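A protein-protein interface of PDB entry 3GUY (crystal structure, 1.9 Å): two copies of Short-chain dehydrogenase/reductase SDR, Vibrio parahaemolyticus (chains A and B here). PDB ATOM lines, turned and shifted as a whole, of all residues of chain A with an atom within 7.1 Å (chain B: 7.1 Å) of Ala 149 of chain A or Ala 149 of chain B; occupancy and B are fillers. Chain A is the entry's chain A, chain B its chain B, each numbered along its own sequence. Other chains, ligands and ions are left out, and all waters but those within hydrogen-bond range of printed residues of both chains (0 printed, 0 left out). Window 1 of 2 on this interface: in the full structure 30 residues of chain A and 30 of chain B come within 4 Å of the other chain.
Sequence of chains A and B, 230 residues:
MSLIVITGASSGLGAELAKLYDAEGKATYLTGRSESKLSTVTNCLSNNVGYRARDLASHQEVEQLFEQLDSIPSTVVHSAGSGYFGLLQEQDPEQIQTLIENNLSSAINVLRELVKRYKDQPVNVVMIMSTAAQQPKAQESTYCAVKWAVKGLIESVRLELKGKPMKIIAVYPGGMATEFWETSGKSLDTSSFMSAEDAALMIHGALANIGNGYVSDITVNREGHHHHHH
Ala 145 of chain A touches Ala 149 of chain B, and with the chains exchanged Ala 149 of chain A touches Ala 145 of chain B. Trp 148 of chain A touches Lys 151 of chain B, and with the chains exchanged Lys 151 of chain A touches Trp 148 of chain B. Trp 148 of chain A touches Gly 152 of chain B, and with the chains exchanged Gly 152 of chain A touches Trp 148 of chain B. Ala 149 of chain B touches its own counterpart, Ala 149 of chain A. Positions printed for both chains: 104, 107, 108, 129, 133, 141, 142, 143, 144, 145, 146, 147, 148, 149, 150, 151, 152, 153, 154 and 155.
Of chain B, only Ala 145 (3.2 Å) and Ala 149 (3.7 Å) come within 4 Å of Ala 149 of chain A. Printed residues of chain A within 4 Å of Ala 145 of chain B: Ala 149. Of the printed residues of chain A, Trp 148 of chain B touches Trp 148, Lys 151 and Gly 152. Of the printed residues of chain A, Ala 149 of chain B touches Ala 145 and Ala 149. The nearest residue of chain B that does not touch Ala 149 of chain A is Trp 148 of chain B (4.4 Å). The nearest residue of chain A that does not touch Ala 149 of chain B is Trp 148 of chain A (4.4 Å). The nearest printed residue of chain B that does not touch Trp 148 of chain A is Ala 149 of chain B (4.4 Å).
Among the printed residues, merely in contact across the chains: Ser 141 of chain A with Leu 153 of chain B, Ala 145 of chain A with Ala 149 of chain B, Trp 148 of chain A with Trp 148 of chain B, Trp 148 of chain A with Lys 151 of chain B, Trp 148 of chain A with Gly 152 of chain B, Ala 149 of chain A with Ala 145 of chain B, Ala 149 of chain A with Ala 149 of chain B, Lys 151 of chain A with Trp 148 of chain B, Gly 152 of chain A with Trp 148 of chain B and Leu 153 of chain A with Ser 141 of chain B.
Printed residues of chain A that touch a printed residue of chain B: Ser 141, Ala 145, Trp 148, Ala 149, Lys 151, Gly 152 and Leu 153. Hydrophobic or aromatic side chains of chain B within 4 Å of the printed part of chain A: Ala 145, Trp 148, Ala 149 and Leu 153.
The side-chain sulfur (SD) of Met 129 of chain A is in hydrogen-bond range of the backbone NH (N) of Lys 151 of chain A, 3.5 Å away. The backbone NH (N) of Lys 151 of chain B sits at hydrogen-bond distance from the side-chain sulfur (SD) of Met 129 of chain B (3.6 Å).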
ATOM      1  N   LEU A 104      14.977  -6.552   9.641  1.00  0.00           N
ATOM      2  CA  LEU A 104      16.013  -6.070   8.751  1.00  0.00           C
ATOM      3  C   LEU A 104      17.284  -5.666   9.532  1.00  0.00           C
ATOM      4  O   LEU A 104      18.400  -6.077   9.158  1.00  0.00           O
ATOM      5  CB  LEU A 104      15.507  -4.898   7.945  1.00  0.00           C
ATOM      6  CG  LEU A 104      16.533  -4.397   6.910  1.00  0.00           C
ATOM      7  CD1 LEU A 104      17.207  -5.518   6.128  1.00  0.00           C
ATOM      8  CD2 LEU A 104      15.851  -3.363   5.984  1.00  0.00           C
ATOM      9  N   ALA A 107      19.111  -8.747  10.923  1.00  0.00           N
ATOM     10  CA  ALA A 107      19.791  -9.515   9.890  1.00  0.00           C
ATOM     11  C   ALA A 107      21.040  -8.781   9.411  1.00  0.00           C
ATOM     12  O   ALA A 107      22.071  -9.395   9.233  1.00  0.00           O
ATOM     13  CB  ALA A 107      18.860  -9.759   8.670  1.00  0.00           C
ATOM     14  N   ILE A 108      20.937  -7.460   9.213  1.00  0.00           N
ATOM     15  CA  ILE A 108      22.096  -6.675   8.791  1.00  0.00           C
ATOM     16  C   ILE A 108      23.230  -6.783   9.845  1.00  0.00           C
ATOM     17  O   ILE A 108      24.374  -7.096   9.508  1.00  0.00           O
ATOM     18  CB  ILE A 108      21.760  -5.207   8.548  1.00  0.00           C
ATOM     19  CG1 ILE A 108      20.883  -5.054   7.292  1.00  0.00           C
ATOM     20  CG2 ILE A 108      23.095  -4.397   8.343  1.00  0.00           C
ATOM     21  CD1 ILE A 108      20.256  -3.656   7.164  1.00  0.00           C
ATOM     22  N   MET A 129      14.306 -16.603   6.373  1.00  0.00           N
ATOM     23  CA  MET A 129      13.508 -15.483   5.891  1.00  0.00           C
ATOM     24  C   MET A 129      12.025 -15.993   5.935  1.00  0.00           C
ATOM     25  O   MET A 129      11.576 -16.382   6.982  1.00  0.00           O
ATOM     26  CB  MET A 129      14.003 -15.121   4.503  1.00  0.00           C
ATOM     27  CG  MET A 129      15.415 -14.458   4.491  1.00  0.00           C
ATOM     28  SD  MET A 129      16.179 -14.112   2.911  1.00  0.00           S
ATOM     29  CE  MET A 129      16.928 -15.738   2.753  1.00  0.00           C
ATOM     30  N   ALA A 133       9.468 -13.377   1.345  1.00  0.00           N
ATOM     31  CA  ALA A 133      10.668 -12.813   0.677  1.00  0.00           C
ATOM     32  C   ALA A 133      10.680 -13.008  -0.830  1.00  0.00           C
ATOM     33  O   ALA A 133      11.466 -12.377  -1.524  1.00  0.00           O
ATOM     34  CB  ALA A 133      11.947 -13.469   1.249  1.00  0.00           C
ATOM     35  N   SER A 141       2.369  -6.052   3.369  1.00  0.00           N
ATOM     36  CA  SER A 141       3.243  -5.217   2.528  1.00  0.00           C
ATOM     37  C   SER A 141       4.541  -4.893   3.225  1.00  0.00           C
ATOM     38  O   SER A 141       5.590  -4.947   2.568  1.00  0.00           O
ATOM     39  CB  SER A 141       2.536  -3.940   2.058  1.00  0.00           C
ATOM     40  OG  SER A 141       2.270  -3.069   3.108  1.00  0.00           O
ATOM     41  N   THR A 142       4.472  -4.570   4.512  1.00  0.00           N
ATOM     42  CA  THR A 142       5.693  -4.215   5.293  1.00  0.00           C
ATOM     43  C   THR A 142       6.498  -5.416   5.724  1.00  0.00           C
ATOM     44  O   THR A 142       7.738  -5.311   5.882  1.00  0.00           O
ATOM     45  CB  THR A 142       5.407  -3.308   6.499  1.00  0.00           C
ATOM     46  OG1 THR A 142       4.418  -3.932   7.322  1.00  0.00           O
ATOM     47  CG2 THR A 142       4.967  -1.869   6.046  1.00  0.00           C
ATOM     48  N   TYR A 143       5.836  -6.558   5.894  1.00  0.00           N
ATOM     49  CA  TYR A 143       6.490  -7.853   6.168  1.00  0.00           C
ATOM     50  C   TYR A 143       7.207  -8.361   4.926  1.00  0.00           C
ATOM     51  O   TYR A 143       8.352  -8.745   4.987  1.00  0.00           O
ATOM     52  CB  TYR A 143       5.488  -8.922   6.661  1.00  0.00           C
ATOM     53  CG  TYR A 143       6.110 -10.226   7.098  1.00  0.00           C
ATOM     54  CD1 TYR A 143       6.868 -10.294   8.263  1.00  0.00           C
ATOM     55  CD2 TYR A 143       5.921 -11.401   6.369  1.00  0.00           C
ATOM     56  CE1 TYR A 143       7.435 -11.486   8.691  1.00  0.00           C
ATOM     57  CE2 TYR A 143       6.480 -12.629   6.790  1.00  0.00           C
ATOM     58  CZ  TYR A 143       7.231 -12.654   7.954  1.00  0.00           C
ATOM     59  OH  TYR A 143       7.828 -13.797   8.372  1.00  0.00           O
ATOM     60  N   CYS A 144       6.528  -8.339   3.771  1.00  0.00           N
ATOM     61  CA  CYS A 144       7.208  -8.560   2.501  1.00  0.00           C
ATOM     62  C   CYS A 144       8.376  -7.595   2.384  1.00  0.00           C
ATOM     63  O   CYS A 144       9.480  -8.016   2.005  1.00  0.00           O
ATOM     64  CB  CYS A 144       6.270  -8.400   1.269  1.00  0.00           C
ATOM     65  SG  CYS A 144       5.059  -9.740   1.308  1.00  0.00           S
ATOM     66  N   ALA A 145       8.154  -6.335   2.715  1.00  0.00           N
ATOM     67  CA  ALA A 145       9.241  -5.354   2.545  1.00  0.00           C
ATOM     68  C   ALA A 145      10.512  -5.778   3.278  1.00  0.00           C
ATOM     69  O   ALA A 145      11.602  -5.762   2.698  1.00  0.00           O
ATOM     70  CB  ALA A 145       8.805  -3.960   2.967  1.00  0.00           C
ATOM     71  N   VAL A 146      10.386  -6.150   4.559  1.00  0.00           N
ATOM     72  CA  VAL A 146      11.553  -6.509   5.348  1.00  0.00           C
ATOM     73  C   VAL A 146      12.151  -7.830   4.963  1.00  0.00           C
ATOM     74  O   VAL A 146      13.377  -7.957   4.992  1.00  0.00           O
ATOM     75  CB  VAL A 146      11.327  -6.402   6.906  1.00  0.00           C
ATOM     76  CG1 VAL A 146      11.024  -4.958   7.302  1.00  0.00           C
ATOM     77  CG2 VAL A 146      10.257  -7.418   7.397  1.00  0.00           C
ATOM     78  N   LYS A 147      11.329  -8.809   4.563  1.00  0.00           N
ATOM     79  CA  LYS A 147      11.817 -10.053   4.036  1.00  0.00           C
ATOM     80  C   LYS A 147      12.479  -9.960   2.679  1.00  0.00           C
ATOM     81  O   LYS A 147      13.569 -10.607   2.462  1.00  0.00           O
ATOM     82  CB  LYS A 147      10.737 -11.148   4.036  1.00  0.00           C
ATOM     83  CG  LYS A 147      10.291 -11.501   5.481  1.00  0.00           C
ATOM     84  CD  LYS A 147      11.417 -12.032   6.364  1.00  0.00           C
ATOM     85  CE  LYS A 147      10.893 -12.430   7.767  1.00  0.00           C
ATOM     86  NZ  LYS A 147      11.901 -12.588   8.787  1.00  0.00           N
ATOM     87  N   TRP A 148      11.906  -9.172   1.754  1.00  0.00           N
ATOM     88  CA  TRP A 148      12.612  -8.917   0.515  1.00  0.00           C
ATOM     89  C   TRP A 148      13.987  -8.267   0.742  1.00  0.00           C
ATOM     90  O   TRP A 148      14.950  -8.576   0.019  1.00  0.00           O
ATOM     91  CB  TRP A 148      11.794  -8.037  -0.453  1.00  0.00           C
ATOM     92  CG  TRP A 148      10.626  -8.702  -1.136  1.00  0.00           C
ATOM     93  CD1 TRP A 148       9.619  -9.525  -0.552  1.00  0.00           C
ATOM     94  CD2 TRP A 148      10.326  -8.639  -2.517  1.00  0.00           C
ATOM     95  NE1 TRP A 148       8.721  -9.913  -1.527  1.00  0.00           N
ATOM     96  CE2 TRP A 148       9.137  -9.415  -2.740  1.00  0.00           C
ATOM     97  CE3 TRP A 148      10.939  -7.997  -3.609  1.00  0.00           C
ATOM     98  CZ2 TRP A 148       8.546  -9.535  -4.014  1.00  0.00           C
ATOM     99  CZ3 TRP A 148      10.353  -8.110  -4.867  1.00  0.00           C
ATOM    100  CH2 TRP A 148       9.174  -8.901  -5.066  1.00  0.00           C
ATOM    101  N   ALA A 149      14.036  -7.362   1.716  1.00  0.00           N
ATOM    102  CA  ALA A 149      15.235  -6.600   2.090  1.00  0.00           C
ATOM    103  C   ALA A 149      16.297  -7.584   2.497  1.00  0.00           C
ATOM    104  O   ALA A 149      17.438  -7.507   2.055  1.00  0.00           O
ATOM    105  CB  ALA A 149      14.872  -5.613   3.257  1.00  0.00           C
ATOM    106  N   VAL A 150      15.919  -8.545   3.337  1.00  0.00           N
ATOM    107  CA  VAL A 150      16.872  -9.537   3.777  1.00  0.00           C
ATOM    108  C   VAL A 150      17.350 -10.387   2.620  1.00  0.00           C
ATOM    109  O   VAL A 150      18.539 -10.635   2.538  1.00  0.00           O
ATOM    110  CB  VAL A 150      16.336 -10.410   4.956  1.00  0.00           C
ATOM    111  CG1 VAL A 150      17.369 -11.496   5.330  1.00  0.00           C
ATOM    112  CG2 VAL A 150      16.021  -9.467   6.178  1.00  0.00           C
ATOM    113  N   LYS A 151      16.470 -10.793   1.687  1.00  0.00           N
ATOM    114  CA  LYS A 151      16.930 -11.568   0.533  1.00  0.00           C
ATOM    115  C   LYS A 151      17.905 -10.769  -0.384  1.00  0.00           C
ATOM    116  O   LYS A 151      18.935 -11.276  -0.797  1.00  0.00           O
ATOM    117  CB  LYS A 151      15.755 -12.051  -0.313  1.00  0.00           C
ATOM    118  CG  LYS A 151      16.154 -12.994  -1.424  1.00  0.00           C
ATOM    119  CD  LYS A 151      14.945 -13.432  -2.259  1.00  0.00           C
ATOM    120  CE  LYS A 151      15.445 -14.172  -3.522  1.00  0.00           C
ATOM    121  NZ  LYS A 151      14.345 -14.579  -4.427  1.00  0.00           N
ATOM    122  N   GLY A 152      17.625  -9.499  -0.592  1.00  0.00           N
ATOM    123  CA  GLY A 152      18.521  -8.602  -1.363  1.00  0.00           C
ATOM    124  C   GLY A 152      19.882  -8.479  -0.704  1.00  0.00           C
ATOM    125  O   GLY A 152      20.946  -8.588  -1.384  1.00  0.00           O
ATOM    126  N   LEU A 153      19.854  -8.271   0.610  1.00  0.00           N
ATOM    127  CA  LEU A 153      21.067  -8.306   1.393  1.00  0.00           C
ATOM    128  C   LEU A 153      21.893  -9.582   1.213  1.00  0.00           C
ATOM    129  O   LEU A 153      23.099  -9.510   0.903  1.00  0.00           O
ATOM    130  CB  LEU A 153      20.737  -8.082   2.846  1.00  0.00           C
ATOM    131  CG  LEU A 153      21.863  -8.178   3.879  1.00  0.00           C
ATOM    132  CD1 LEU A 153      22.629  -6.813   3.867  1.00  0.00           C
ATOM    133  CD2 LEU A 153      21.366  -8.546   5.378  1.00  0.00           C
ATOM    134  N   ILE A 154      21.293 -10.751   1.447  1.00  0.00           N
ATOM    135  CA  ILE A 154      22.065 -12.007   1.386  1.00  0.00           C
ATOM    136  C   ILE A 154      22.529 -12.357  -0.012  1.00  0.00           C
ATOM    137  O   ILE A 154      23.657 -12.838  -0.176  1.00  0.00           O
ATOM    138  CB  ILE A 154      21.380 -13.182   2.091  1.00  0.00           C
ATOM    139  CG1 ILE A 154      20.089 -13.631   1.372  1.00  0.00           C
ATOM    140  CG2 ILE A 154      21.085 -12.814   3.542  1.00  0.00           C
ATOM    141  CD1 ILE A 154      20.267 -14.903   0.648  1.00  0.00           C
ATOM    142  N   GLU A 155      21.708 -12.054  -1.028  1.00  0.00           N
ATOM    143  CA  GLU A 155      22.123 -12.334  -2.382  1.00  0.00           C
ATOM    144  C   GLU A 155      23.312 -11.472  -2.775  1.00  0.00           C
ATOM    145  O   GLU A 155      24.201 -11.976  -3.458  1.00  0.00           O
ATOM    146  CB  GLU A 155      21.002 -12.189  -3.364  1.00  0.00           C
ATOM    147  CG  GLU A 155      19.869 -13.213  -3.109  1.00  0.00           C
ATOM    148  CD  GLU A 155      20.225 -14.623  -3.482  1.00  0.00           C
ATOM    149  OE1 GLU A 155      21.429 -14.925  -3.599  1.00  0.00           O
ATOM    150  OE2 GLU A 155      19.279 -15.455  -3.643  1.00  0.00           O
ATOM    151  N   LEU B 104      13.794   3.341   2.867  1.00  0.00           N
ATOM    152  CA  LEU B 104      12.674   2.445   3.160  1.00  0.00           C
ATOM    153  C   LEU B 104      11.588   3.131   4.026  1.00  0.00           C
ATOM    154  O   LEU B 104      10.411   3.158   3.624  1.00  0.00           O
ATOM    155  CB  LEU B 104      13.177   1.192   3.827  1.00  0.00           C
ATOM    156  CG  LEU B 104      12.098   0.184   4.303  1.00  0.00           C
ATOM    157  CD1 LEU B 104      11.109  -0.181   3.171  1.00  0.00           C
ATOM    158  CD2 LEU B 104      12.762  -1.010   4.972  1.00  0.00           C
ATOM    159  N   ALA B 107       9.728   5.691   1.889  1.00  0.00           N
ATOM    160  CA  ALA B 107       8.808   5.089   0.942  1.00  0.00           C
ATOM    161  C   ALA B 107       7.548   4.604   1.665  1.00  0.00           C
ATOM    162  O   ALA B 107       6.453   4.790   1.135  1.00  0.00           O
ATOM    163  CB  ALA B 107       9.448   3.949   0.183  1.00  0.00           C
ATOM    164  N   ILE B 108       7.712   3.935   2.814  1.00  0.00           N
ATOM    165  CA  ILE B 108       6.587   3.396   3.573  1.00  0.00           C
ATOM    166  C   ILE B 108       5.691   4.520   4.053  1.00  0.00           C
ATOM    167  O   ILE B 108       4.510   4.475   3.897  1.00  0.00           O
ATOM    168  CB  ILE B 108       7.023   2.631   4.836  1.00  0.00           C
ATOM    169  CG1 ILE B 108       7.674   1.309   4.457  1.00  0.00           C
ATOM    170  CG2 ILE B 108       5.804   2.428   5.782  1.00  0.00           C
ATOM    171  CD1 ILE B 108       8.452   0.698   5.593  1.00  0.00           C
ATOM    172  N   MET B 129      12.781   3.798  -7.695  1.00  0.00           N
ATOM    173  CA  MET B 129      13.618   2.880  -6.915  1.00  0.00           C
ATOM    174  C   MET B 129      15.017   2.870  -7.540  1.00  0.00           C
ATOM    175  O   MET B 129      15.682   3.873  -7.536  1.00  0.00           O
ATOM    176  CB  MET B 129      12.973   1.462  -6.803  1.00  0.00           C
ATOM    177  CG  MET B 129      11.653   1.396  -5.959  1.00  0.00           C
ATOM    178  SD  MET B 129      10.760  -0.165  -6.070  1.00  0.00           S
ATOM    179  CE  MET B 129       9.782   0.356  -7.521  1.00  0.00           C
ATOM    180  N   ALA B 133      17.022  -2.671  -6.989  1.00  0.00           N
ATOM    181  CA  ALA B 133      15.811  -3.378  -6.507  1.00  0.00           C
ATOM    182  C   ALA B 133      15.579  -4.711  -7.202  1.00  0.00           C
ATOM    183  O   ALA B 133      14.839  -5.537  -6.692  1.00  0.00           O
ATOM    184  CB  ALA B 133      14.539  -2.472  -6.724  1.00  0.00           C
ATOM    185  N   SER B 141      25.246  -4.165  -0.773  1.00  0.00           N
ATOM    186  CA  SER B 141      24.325  -5.062  -0.059  1.00  0.00           C
ATOM    187  C   SER B 141      23.175  -4.377   0.668  1.00  0.00           C
ATOM    188  O   SER B 141      22.038  -4.808   0.523  1.00  0.00           O
ATOM    189  CB  SER B 141      25.072  -6.011   0.852  1.00  0.00           C
ATOM    190  OG  SER B 141      25.732  -5.392   1.900  1.00  0.00           O
ATOM    191  N   THR B 142      23.449  -3.291   1.386  1.00  0.00           N
ATOM    192  CA  THR B 142      22.428  -2.563   2.124  1.00  0.00           C
ATOM    193  C   THR B 142      21.584  -1.687   1.238  1.00  0.00           C
ATOM    194  O   THR B 142      20.399  -1.469   1.523  1.00  0.00           O
ATOM    195  CB  THR B 142      23.025  -1.791   3.299  1.00  0.00           C
ATOM    196  OG1 THR B 142      24.076  -0.911   2.849  1.00  0.00           O
ATOM    197  CG2 THR B 142      23.576  -2.756   4.333  1.00  0.00           C
ATOM    198  N   TYR B 143      22.157  -1.203   0.152  1.00  0.00           N
ATOM    199  CA  TYR B 143      21.399  -0.452  -0.853  1.00  0.00           C
ATOM    200  C   TYR B 143      20.415  -1.349  -1.598  1.00  0.00           C
ATOM    201  O   TYR B 143      19.243  -1.010  -1.747  1.00  0.00           O
ATOM    202  CB  TYR B 143      22.372   0.264  -1.821  1.00  0.00           C
ATOM    203  CG  TYR B 143      21.717   1.208  -2.783  1.00  0.00           C
ATOM    204  CD1 TYR B 143      21.198   2.429  -2.339  1.00  0.00           C
ATOM    205  CD2 TYR B 143      21.618   0.904  -4.136  1.00  0.00           C
ATOM    206  CE1 TYR B 143      20.596   3.339  -3.237  1.00  0.00           C
ATOM    207  CE2 TYR B 143      21.028   1.773  -5.025  1.00  0.00           C
ATOM    208  CZ  TYR B 143      20.499   2.986  -4.563  1.00  0.00           C
ATOM    209  OH  TYR B 143      19.897   3.859  -5.438  1.00  0.00           O
ATOM    210  N   CYS B 144      20.902  -2.509  -2.048  1.00  0.00           N
ATOM    211  CA  CYS B 144      20.032  -3.588  -2.517  1.00  0.00           C
ATOM    212  C   CYS B 144      18.947  -3.903  -1.489  1.00  0.00           C
ATOM    213  O   CYS B 144      17.777  -3.897  -1.816  1.00  0.00           O
ATOM    214  CB  CYS B 144      20.805  -4.822  -2.909  1.00  0.00           C
ATOM    215  SG  CYS B 144      21.747  -4.495  -4.411  1.00  0.00           S
ATOM    216  N   ALA B 145      19.335  -4.083  -0.229  1.00  0.00           N
ATOM    217  CA  ALA B 145      18.346  -4.386   0.810  1.00  0.00           C
ATOM    218  C   ALA B 145      17.194  -3.392   0.837  1.00  0.00           C
ATOM    219  O   ALA B 145      16.045  -3.814   0.813  1.00  0.00           O
ATOM    220  CB  ALA B 145      19.008  -4.484   2.161  1.00  0.00           C
ATOM    221  N   VAL B 146      17.488  -2.084   0.855  1.00  0.00           N
ATOM    222  CA  VAL B 146      16.481  -1.065   0.968  1.00  0.00           C
ATOM    223  C   VAL B 146      15.667  -0.919  -0.305  1.00  0.00           C
ATOM    224  O   VAL B 146      14.466  -0.650  -0.213  1.00  0.00           O
ATOM    225  CB  VAL B 146      17.015   0.303   1.493  1.00  0.00           C
ATOM    226  CG1 VAL B 146      17.646   0.145   2.904  1.00  0.00           C
ATOM    227  CG2 VAL B 146      18.006   0.967   0.499  1.00  0.00           C
ATOM    228  N   LYS B 147      16.287  -1.118  -1.468  1.00  0.00           N
ATOM    229  CA  LYS B 147      15.560  -1.026  -2.740  1.00  0.00           C
ATOM    230  C   LYS B 147      14.670  -2.251  -3.015  1.00  0.00           C
ATOM    231  O   LYS B 147      13.526  -2.105  -3.531  1.00  0.00           O
ATOM    232  CB  LYS B 147      16.533  -0.737  -3.906  1.00  0.00           C
ATOM    233  CG  LYS B 147      17.272   0.629  -3.761  1.00  0.00           C
ATOM    234  CD  LYS B 147      16.298   1.784  -3.635  1.00  0.00           C
ATOM    235  CE  LYS B 147      16.908   3.178  -3.826  1.00  0.00           C
ATOM    236  NZ  LYS B 147      15.922   4.259  -3.511  1.00  0.00           N
ATOM    237  N   TRP B 148      15.191  -3.444  -2.739  1.00  0.00           N
ATOM    238  CA  TRP B 148      14.368  -4.667  -2.764  1.00  0.00           C
ATOM    239  C   TRP B 148      13.146  -4.480  -1.823  1.00  0.00           C
ATOM    240  O   TRP B 148      12.012  -4.871  -2.142  1.00  0.00           O
ATOM    241  CB  TRP B 148      15.184  -5.876  -2.298  1.00  0.00           C
ATOM    242  CG  TRP B 148      16.067  -6.414  -3.276  1.00  0.00           C
ATOM    243  CD1 TRP B 148      17.043  -5.753  -3.984  1.00  0.00           C
ATOM    244  CD2 TRP B 148      16.106  -7.768  -3.726  1.00  0.00           C
ATOM    245  NE1 TRP B 148      17.663  -6.595  -4.838  1.00  0.00           N
ATOM    246  CE2 TRP B 148      17.135  -7.851  -4.691  1.00  0.00           C
ATOM    247  CE3 TRP B 148      15.373  -8.919  -3.400  1.00  0.00           C
ATOM    248  CZ2 TRP B 148      17.463  -9.039  -5.344  1.00  0.00           C
ATOM    249  CZ3 TRP B 148      15.720 -10.138  -4.048  1.00  0.00           C
ATOM    250  CH2 TRP B 148      16.753 -10.174  -5.006  1.00  0.00           C
ATOM    251  N   ALA B 149      13.395  -3.947  -0.634  1.00  0.00           N
ATOM    252  CA  ALA B 149      12.312  -3.735   0.359  1.00  0.00           C
ATOM    253  C   ALA B 149      11.181  -2.871  -0.226  1.00  0.00           C
ATOM    254  O   ALA B 149      10.017  -3.191  -0.083  1.00  0.00           O
ATOM    255  CB  ALA B 149      12.862  -3.031   1.638  1.00  0.00           C
ATOM    256  N   VAL B 150      11.542  -1.748  -0.832  1.00  0.00           N
ATOM    257  CA  VAL B 150      10.547  -0.894  -1.445  1.00  0.00           C
ATOM    258  C   VAL B 150       9.793  -1.623  -2.557  1.00  0.00           C
ATOM    259  O   VAL B 150       8.583  -1.437  -2.677  1.00  0.00           O
ATOM    260  CB  VAL B 150      11.120   0.508  -1.956  1.00  0.00           C
ATOM    261  CG1 VAL B 150      10.004   1.314  -2.681  1.00  0.00           C
ATOM    262  CG2 VAL B 150      11.697   1.352  -0.807  1.00  0.00           C
ATOM    263  N   LYS B 151      10.447  -2.476  -3.343  1.00  0.00           N
ATOM    264  CA  LYS B 151       9.764  -3.211  -4.392  1.00  0.00           C
ATOM    265  C   LYS B 151       8.810  -4.261  -3.757  1.00  0.00           C
ATOM    266  O   LYS B 151       7.652  -4.376  -4.166  1.00  0.00           O
ATOM    267  CB  LYS B 151      10.754  -3.896  -5.326  1.00  0.00           C
ATOM    268  CG  LYS B 151      10.095  -4.600  -6.549  1.00  0.00           C
ATOM    269  CD  LYS B 151      11.096  -5.389  -7.411  1.00  0.00           C
ATOM    270  CE  LYS B 151      10.394  -6.298  -8.474  1.00  0.00           C
ATOM    271  NZ  LYS B 151      11.427  -6.628  -9.427  1.00  0.00           N
ATOM    272  N   GLY B 152       9.265  -4.975  -2.730  1.00  0.00           N
ATOM    273  CA  GLY B 152       8.330  -5.821  -2.004  1.00  0.00           C
ATOM    274  C   GLY B 152       7.098  -5.055  -1.482  1.00  0.00           C
ATOM    275  O   GLY B 152       5.990  -5.564  -1.600  1.00  0.00           O
ATOM    276  N   LEU B 153       7.299  -3.869  -0.914  1.00  0.00           N
ATOM    277  CA  LEU B 153       6.223  -3.003  -0.416  1.00  0.00           C
ATOM    278  C   LEU B 153       5.235  -2.685  -1.552  1.00  0.00           C
ATOM    279  O   LEU B 153       4.034  -2.947  -1.407  1.00  0.00           O
ATOM    280  CB  LEU B 153       6.767  -1.718   0.169  1.00  0.00           C
ATOM    281  CG  LEU B 153       5.776  -0.698   0.645  1.00  0.00           C
ATOM    282  CD1 LEU B 153       5.122  -1.153   1.979  1.00  0.00           C
ATOM    283  CD2 LEU B 153       6.482   0.700   0.817  1.00  0.00           C
ATOM    284  N   ILE B 154       5.736  -2.156  -2.671  1.00  0.00           N
ATOM    285  CA  ILE B 154       4.825  -1.683  -3.723  1.00  0.00           C
ATOM    286  C   ILE B 154       4.077  -2.817  -4.443  1.00  0.00           C
ATOM    287  O   ILE B 154       2.913  -2.648  -4.819  1.00  0.00           O
ATOM    288  CB  ILE B 154       5.473  -0.673  -4.708  1.00  0.00           C
ATOM    289  CG1 ILE B 154       6.477  -1.335  -5.654  1.00  0.00           C
ATOM    290  CG2 ILE B 154       6.076   0.529  -3.901  1.00  0.00           C
ATOM    291  CD1 ILE B 154       5.880  -1.786  -7.047  1.00  0.00           C
ATOM    292  N   GLU B 155       4.731  -3.950  -4.635  1.00  0.00           N
ATOM    293  CA  GLU B 155       4.100  -5.063  -5.303  1.00  0.00           C
ATOM    294  C   GLU B 155       2.999  -5.670  -4.435  1.00  0.00           C
ATOM    295  O   GLU B 155       2.013  -6.219  -4.983  1.00  0.00           O
ATOM    296  CB  GLU B 155       5.112  -6.109  -5.698  1.00  0.00           C
ATOM    297  CG  GLU B 155       6.210  -5.640  -6.737  1.00  0.00           C
ATOM    298  CD  GLU B 155       5.698  -5.467  -8.162  1.00  0.00           C
ATOM    299  OE1 GLU B 155       4.447  -5.315  -8.336  1.00  0.00           O
ATOM    300  OE2 GLU B 155       6.547  -5.461  -9.109  1.00  0.00           O
